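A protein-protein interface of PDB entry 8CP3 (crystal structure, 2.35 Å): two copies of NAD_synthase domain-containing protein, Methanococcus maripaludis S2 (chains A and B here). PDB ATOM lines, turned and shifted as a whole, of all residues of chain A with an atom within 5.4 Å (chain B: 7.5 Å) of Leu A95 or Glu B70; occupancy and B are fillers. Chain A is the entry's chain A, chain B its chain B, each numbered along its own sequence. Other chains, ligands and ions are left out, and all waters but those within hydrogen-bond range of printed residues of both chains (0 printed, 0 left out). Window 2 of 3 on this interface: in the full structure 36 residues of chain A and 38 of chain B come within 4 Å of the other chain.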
ATOM      1  N   ASN A  65      27.179  13.507  17.957  1.00  0.00           N
ATOM      2  CA  ASN A  65      25.791  13.627  17.519  1.00  0.00           C
ATOM      3  C   ASN A  65      25.459  14.979  16.905  1.00  0.00           C
ATOM      4  O   ASN A  65      24.281  15.259  16.694  1.00  0.00           O
ATOM      5  CB  ASN A  65      24.833  13.373  18.683  1.00  0.00           C
ATOM      6  CG  ASN A  65      25.045  14.347  19.822  1.00  0.00           C
ATOM      7  OD1 ASN A  65      25.932  15.212  19.768  1.00  0.00           O
ATOM      8  ND2 ASN A  65      24.242  14.209  20.866  1.00  0.00           N
ATOM      9  N   GLY A  66      26.445  15.843  16.686  1.00  0.00           N
ATOM     10  CA  GLY A  66      26.236  17.180  16.174  1.00  0.00           C
ATOM     11  C   GLY A  66      26.033  18.274  17.209  1.00  0.00           C
ATOM     12  O   GLY A  66      25.934  19.446  16.832  1.00  0.00           O
ATOM     13  N   PHE A  67      26.033  17.957  18.498  1.00  0.00           N
ATOM     14  CA  PHE A  67      25.924  19.004  19.506  1.00  0.00           C
ATOM     15  C   PHE A  67      27.269  19.401  20.096  1.00  0.00           C
ATOM     16  O   PHE A  67      27.325  20.333  20.901  1.00  0.00           O
ATOM     17  CB  PHE A  67      24.935  18.585  20.603  1.00  0.00           C
ATOM     18  CG  PHE A  67      23.523  18.496  20.114  1.00  0.00           C
ATOM     19  CD1 PHE A  67      23.087  17.383  19.410  1.00  0.00           C
ATOM     20  CD2 PHE A  67      22.653  19.559  20.277  1.00  0.00           C
ATOM     21  CE1 PHE A  67      21.795  17.316  18.922  1.00  0.00           C
ATOM     22  CE2 PHE A  67      21.349  19.500  19.778  1.00  0.00           C
ATOM     23  CZ  PHE A  67      20.925  18.371  19.099  1.00  0.00           C
ATOM     24  N   PHE A  68      28.352  18.766  19.668  1.00  0.00           N
ATOM     25  CA  PHE A  68      29.700  19.124  20.081  1.00  0.00           C
ATOM     26  C   PHE A  68      30.489  19.606  18.872  1.00  0.00           C
ATOM     27  O   PHE A  68      30.502  18.935  17.838  1.00  0.00           O
ATOM     28  CB  PHE A  68      30.384  17.921  20.701  1.00  0.00           C
ATOM     29  CG  PHE A  68      29.740  17.446  21.962  1.00  0.00           C
ATOM     30  CD1 PHE A  68      30.167  17.934  23.191  1.00  0.00           C
ATOM     31  CD2 PHE A  68      28.671  16.543  21.917  1.00  0.00           C
ATOM     32  CE1 PHE A  68      29.574  17.498  24.370  1.00  0.00           C
ATOM     33  CE2 PHE A  68      28.057  16.107  23.084  1.00  0.00           C
ATOM     34  CZ  PHE A  68      28.515  16.586  24.322  1.00  0.00           C
ATOM     35  N   LYS A  91      30.384   8.707  15.151  1.00  0.00           N
ATOM     36  CA  LYS A  91      29.500   9.749  14.656  1.00  0.00           C
ATOM     37  C   LYS A  91      28.131   9.137  14.358  1.00  0.00           C
ATOM     38  O   LYS A  91      28.042   8.049  13.779  1.00  0.00           O
ATOM     39  CB  LYS A  91      30.093  10.432  13.415  1.00  0.00           C
ATOM     40  CG  LYS A  91      29.282  11.637  12.968  1.00  0.00           C
ATOM     41  CD  LYS A  91      29.945  12.422  11.849  1.00  0.00           C
ATOM     42  CE  LYS A  91      29.150  13.708  11.567  1.00  0.00           C
ATOM     43  NZ  LYS A  91      29.230  14.690  12.711  1.00  0.00           N
ATOM     44  N   ASP A  93      24.187  10.521  12.917  1.00  0.00           N
ATOM     45  CA  ASP A  93      23.450  11.658  12.400  1.00  0.00           C
ATOM     46  C   ASP A  93      22.114  11.737  13.126  1.00  0.00           C
ATOM     47  O   ASP A  93      21.057  11.376  12.602  1.00  0.00           O
ATOM     48  CB  ASP A  93      23.305  11.569  10.886  1.00  0.00           C
ATOM     49  CG  ASP A  93      22.816  10.221  10.424  1.00  0.00           C
ATOM     50  OD1 ASP A  93      22.694   9.298  11.262  1.00  0.00           O
ATOM     51  OD2 ASP A  93      22.527  10.103   9.211  1.00  0.00           O
ATOM     52  N   TYR A  94      22.202  12.197  14.380  1.00  0.00           N
ATOM     53  CA  TYR A  94      21.018  12.355  15.219  1.00  0.00           C
ATOM     54  C   TYR A  94      20.124  13.501  14.727  1.00  0.00           C
ATOM     55  O   TYR A  94      18.892  13.400  14.779  1.00  0.00           O
ATOM     56  CB  TYR A  94      21.436  12.570  16.678  1.00  0.00           C
ATOM     57  CG  TYR A  94      20.265  12.730  17.612  1.00  0.00           C
ATOM     58  CD1 TYR A  94      19.340  11.708  17.769  1.00  0.00           C
ATOM     59  CD2 TYR A  94      20.065  13.909  18.316  1.00  0.00           C
ATOM     60  CE1 TYR A  94      18.242  11.848  18.612  1.00  0.00           C
ATOM     61  CE2 TYR A  94      18.972  14.058  19.152  1.00  0.00           C
ATOM     62  CZ  TYR A  94      18.066  13.024  19.308  1.00  0.00           C
ATOM     63  OH  TYR A  94      16.969  13.169  20.134  1.00  0.00           O
ATOM     64  N   LEU A  95      20.724  14.595  14.240  1.00  0.00           N
ATOM     65  CA  LEU A  95      19.950  15.776  13.868  1.00  0.00           C
ATOM     66  C   LEU A  95      18.844  15.447  12.874  1.00  0.00           C
ATOM     67  O   LEU A  95      17.791  16.097  12.880  1.00  0.00           O
ATOM     68  CB  LEU A  95      20.857  16.864  13.295  1.00  0.00           C
ATOM     69  CG  LEU A  95      21.849  17.529  14.260  1.00  0.00           C
ATOM     70  CD1 LEU A  95      22.424  18.775  13.620  1.00  0.00           C
ATOM     71  CD2 LEU A  95      21.225  17.833  15.603  1.00  0.00           C
ATOM     72  N   ASN A  96      19.070  14.458  12.003  1.00  0.00           N
ATOM     73  CA  ASN A  96      18.101  14.066  10.986  1.00  0.00           C
ATOM     74  C   ASN A  96      16.909  13.297  11.553  1.00  0.00           C
ATOM     75  O   ASN A  96      15.953  13.064  10.807  1.00  0.00           O
ATOM     76  CB  ASN A  96      18.786  13.241   9.895  1.00  0.00           C
ATOM     77  CG  ASN A  96      18.188  13.480   8.512  1.00  0.00           C
ATOM     78  OD1 ASN A  96      17.664  14.563   8.225  1.00  0.00           O
ATOM     79  ND2 ASN A  96      18.271  12.473   7.645  1.00  0.00           N
ATOM     80  N   GLU A  97      16.954  12.877  12.822  1.00  0.00           N
ATOM     81  CA  GLU A  97      15.880  12.123  13.476  1.00  0.00           C
ATOM     82  C   GLU A  97      15.017  12.995  14.399  1.00  0.00           C
ATOM     83  O   GLU A  97      15.532  13.596  15.351  1.00  0.00           O
ATOM     84  CB  GLU A  97      16.477  10.950  14.256  1.00  0.00           C
ATOM     85  N   ILE A  98      13.717  13.091  14.094  1.00  0.00           N
ATOM     86  CA  ILE A  98      12.745  13.804  14.933  1.00  0.00           C
ATOM     87  C   ILE A  98      12.092  12.809  15.895  1.00  0.00           C
ATOM     88  O   ILE A  98      11.155  12.097  15.521  1.00  0.00           O
ATOM     89  CB  ILE A  98      11.691  14.513  14.082  1.00  0.00           C
ATOM     90  CG1 ILE A  98      12.356  15.464  13.071  1.00  0.00           C
ATOM     91  CG2 ILE A  98      10.636  15.204  14.971  1.00  0.00           C
ATOM     92  CD1 ILE A  98      13.230  16.548  13.702  1.00  0.00           C
ATOM     93  N   ASP B  64      32.539  28.708   9.365  1.00  0.00           N
ATOM     94  CA  ASP B  64      32.628  27.474  10.122  1.00  0.00           C
ATOM     95  C   ASP B  64      34.103  27.123  10.263  1.00  0.00           C
ATOM     96  O   ASP B  64      34.712  26.572   9.341  1.00  0.00           O
ATOM     97  CB  ASP B  64      31.823  26.400   9.406  1.00  0.00           C
ATOM     98  CG  ASP B  64      31.976  25.004  10.016  1.00  0.00           C
ATOM     99  OD1 ASP B  64      32.570  24.800  11.115  1.00  0.00           O
ATOM    100  OD2 ASP B  64      31.466  24.089   9.348  1.00  0.00           O
ATOM    101  N   PHE B  68      32.056  25.969  16.142  1.00  0.00           N
ATOM    102  CA  PHE B  68      30.604  25.928  16.247  1.00  0.00           C
ATOM    103  C   PHE B  68      30.129  24.543  15.823  1.00  0.00           C
ATOM    104  O   PHE B  68      30.526  24.053  14.761  1.00  0.00           O
ATOM    105  CB  PHE B  68      29.986  27.006  15.361  1.00  0.00           C
ATOM    106  CG  PHE B  68      30.394  28.400  15.738  1.00  0.00           C
ATOM    107  CD1 PHE B  68      29.641  29.145  16.633  1.00  0.00           C
ATOM    108  CD2 PHE B  68      31.591  28.939  15.247  1.00  0.00           C
ATOM    109  CE1 PHE B  68      30.040  30.428  16.993  1.00  0.00           C
ATOM    110  CE2 PHE B  68      32.011  30.220  15.611  1.00  0.00           C
ATOM    111  CZ  PHE B  68      31.227  30.968  16.484  1.00  0.00           C
ATOM    112  N   SER B  69      29.278  23.924  16.637  1.00  0.00           N
ATOM    113  CA  SER B  69      28.736  22.611  16.314  1.00  0.00           C
ATOM    114  C   SER B  69      27.790  22.694  15.118  1.00  0.00           C
ATOM    115  O   SER B  69      27.346  23.774  14.719  1.00  0.00           O
ATOM    116  CB  SER B  69      27.973  22.028  17.510  1.00  0.00           C
ATOM    117  OG  SER B  69      26.797  22.784  17.761  1.00  0.00           O
ATOM    118  N   GLU B  70      27.493  21.524  14.540  1.00  0.00           N
ATOM    119  CA  GLU B  70      26.525  21.438  13.448  1.00  0.00           C
ATOM    120  C   GLU B  70      25.159  21.969  13.868  1.00  0.00           C
ATOM    121  O   GLU B  70      24.526  22.735  13.133  1.00  0.00           O
ATOM    122  CB  GLU B  70      26.423  19.993  12.971  1.00  0.00           C
ATOM    123  CG  GLU B  70      26.035  19.832  11.501  1.00  0.00           C
ATOM    124  CD  GLU B  70      25.598  18.407  11.150  1.00  0.00           C
ATOM    125  OE1 GLU B  70      26.235  17.446  11.644  1.00  0.00           O
ATOM    126  OE2 GLU B  70      24.630  18.248  10.367  1.00  0.00           O
ATOM    127  N   ASN B  71      24.700  21.599  15.069  1.00  0.00           N
ATOM    128  CA  ASN B  71      23.400  22.068  15.553  1.00  0.00           C
ATOM    129  C   ASN B  71      23.325  23.597  15.550  1.00  0.00           C
ATOM    130  O   ASN B  71      22.360  24.192  15.050  1.00  0.00           O
ATOM    131  CB  ASN B  71      23.149  21.488  16.948  1.00  0.00           C
ATOM    132  CG  ASN B  71      21.875  22.005  17.589  1.00  0.00           C
ATOM    133  OD1 ASN B  71      20.758  21.685  17.173  1.00  0.00           O
ATOM    134  ND2 ASN B  71      22.047  22.776  18.650  1.00  0.00           N
ATOM    135  N   VAL B  72      24.372  24.252  16.046  1.00  0.00           N
ATOM    136  CA  VAL B  72      24.405  25.710  16.054  1.00  0.00           C
ATOM    137  C   VAL B  72      24.399  26.258  14.626  1.00  0.00           C
ATOM    138  O   VAL B  72      23.662  27.201  14.311  1.00  0.00           O
ATOM    139  CB  VAL B  72      25.624  26.198  16.862  1.00  0.00           C
ATOM    140  CG1 VAL B  72      25.856  27.687  16.706  1.00  0.00           C
ATOM    141  CG2 VAL B  72      25.471  25.818  18.330  1.00  0.00           C
ATOM    142  N   ILE B  73      25.224  25.678  13.743  1.00  0.00           N
ATOM    143  CA  ILE B  73      25.276  26.109  12.341  1.00  0.00           C
ATOM    144  C   ILE B  73      23.926  25.906  11.663  1.00  0.00           C
ATOM    145  O   ILE B  73      23.457  26.763  10.906  1.00  0.00           O
ATOM    146  CB  ILE B  73      26.394  25.372  11.586  1.00  0.00           C
ATOM    147  CG1 ILE B  73      27.758  25.791  12.125  1.00  0.00           C
ATOM    148  CG2 ILE B  73      26.304  25.617  10.079  1.00  0.00           C
ATOM    149  CD1 ILE B  73      28.925  25.161  11.385  1.00  0.00           C
ATOM    150  N   LYS B  74      23.313  24.742  11.878  1.00  0.00           N
ATOM    151  CA  LYS B  74      22.011  24.473  11.280  1.00  0.00           C
ATOM    152  C   LYS B  74      20.956  25.461  11.776  1.00  0.00           C
ATOM    153  O   LYS B  74      20.110  25.928  11.002  1.00  0.00           O
ATOM    154  CB  LYS B  74      21.596  23.046  11.593  1.00  0.00           C
ATOM    155  CG  LYS B  74      21.114  22.272  10.409  1.00  0.00           C
ATOM    156  CD  LYS B  74      22.284  21.614   9.703  1.00  0.00           C
ATOM    157  CE  LYS B  74      21.805  20.558   8.704  1.00  0.00           C
ATOM    158  NZ  LYS B  74      22.908  19.679   8.198  1.00  0.00           N
ATOM    159  N   LYS B  75      20.982  25.778  13.068  1.00  0.00           N
ATOM    160  CA  LYS B  75      20.012  26.712  13.610  1.00  0.00           C
ATOM    161  C   LYS B  75      20.222  28.093  13.018  1.00  0.00           C
ATOM    162  O   LYS B  75      19.252  28.792  12.702  1.00  0.00           O
ATOM    163  CB  LYS B  75      20.116  26.735  15.140  1.00  0.00           C
ATOM    164  CG  LYS B  75      19.394  25.533  15.795  1.00  0.00           C
ATOM    165  CD  LYS B  75      19.542  25.455  17.323  1.00  0.00           C
ATOM    166  CE  LYS B  75      19.540  26.808  18.007  1.00  0.00           C
ATOM    167  NZ  LYS B  75      18.749  26.757  19.283  1.00  0.00           N
ATOM    168  N   ALA B  76      21.480  28.489  12.812  1.00  0.00           N
ATOM    169  CA  ALA B  76      21.724  29.793  12.214  1.00  0.00           C
ATOM    170  C   ALA B  76      21.207  29.830  10.778  1.00  0.00           C
ATOM    171  O   ALA B  76      20.551  30.795  10.377  1.00  0.00           O
ATOM    172  CB  ALA B  76      23.213  30.131  12.277  1.00  0.00           C
ATOM    173  N   GLU B  77      21.433  28.758  10.018  1.00  0.00           N
ATOM    174  CA  GLU B  77      20.958  28.696   8.638  1.00  0.00           C
ATOM    175  C   GLU B  77      19.437  28.750   8.572  1.00  0.00           C
ATOM    176  O   GLU B  77      18.867  29.502   7.768  1.00  0.00           O
ATOM    177  CB  GLU B  77      21.497  27.433   7.960  1.00  0.00           C
ATOM    178  CG  GLU B  77      23.003  27.515   7.729  1.00  0.00           C
ATOM    179  CD  GLU B  77      23.596  26.200   7.284  1.00  0.00           C
ATOM    180  OE1 GLU B  77      22.889  25.176   7.370  1.00  0.00           O
ATOM    181  OE2 GLU B  77      24.777  26.179   6.867  1.00  0.00           O
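Among the printed residues, pairs that only touch across the chains: Gly A66 with Ser B69, Phe A67 with Ser B69, Phe A67 with Asn B71, Phe A68 with Ser B69, Leu A95 with Glu B70 and Leu A95 with Asn B71.
O of Gly A66 sits at hydrogen-bond distance from N of Glu B70, 3.5 Å away. O of Gly A66 is in hydrogen-bond range of N of Asn B71 (3.0 Å).
Leu A95 touches just these residues of chain B: Glu B70 (3.97 Å) and Asn B71 (3.9 Å). Of chain A, only Gly A66 and Leu A95 come within 4 Å of Glu B70. Of the printed residues of chain A, Ser B69 touches Gly A66 (3.4 Å), Phe A67 (3.8 Å) and Phe A68 (3.7 Å). Printed residues of chain B within 4 Å of Phe A68: Ser B69. Lys B74 touches none of the printed residues of chain A. The nearest residue of chain B that does not touch Leu A95 is Lys B74 (4.8 Å). The nearest residue of chain A that does not touch Glu B70 is Lys A91 (4.2 Å).
The backbone NH of Phe A67 lies within hydrogen-bond range of the side-chain amide oxygen of Asn A65, at 3.0 Å. The side-chain hydroxyl (OG) of Ser B69 lies within hydrogen-bond range of the backbone NH (N) of Val B72. The side-chain carboxylate (OE2) of Glu B70 lies within salt-bridge range of the side-chain amino group (NZ) of Lys B74 (3.1 Å).
Position printed for both chains: 68. Of the 8 pairs that touch across the chains among the printed residues, none has its exchanged pair printed and touching as well.
Of the 11 printed residues of chain B, 3 touch a printed residue of chain A. Hydrophobic or aromatic side chains of chain A within 4 Å of the printed part of chain B: Phe A67 and Leu A95.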
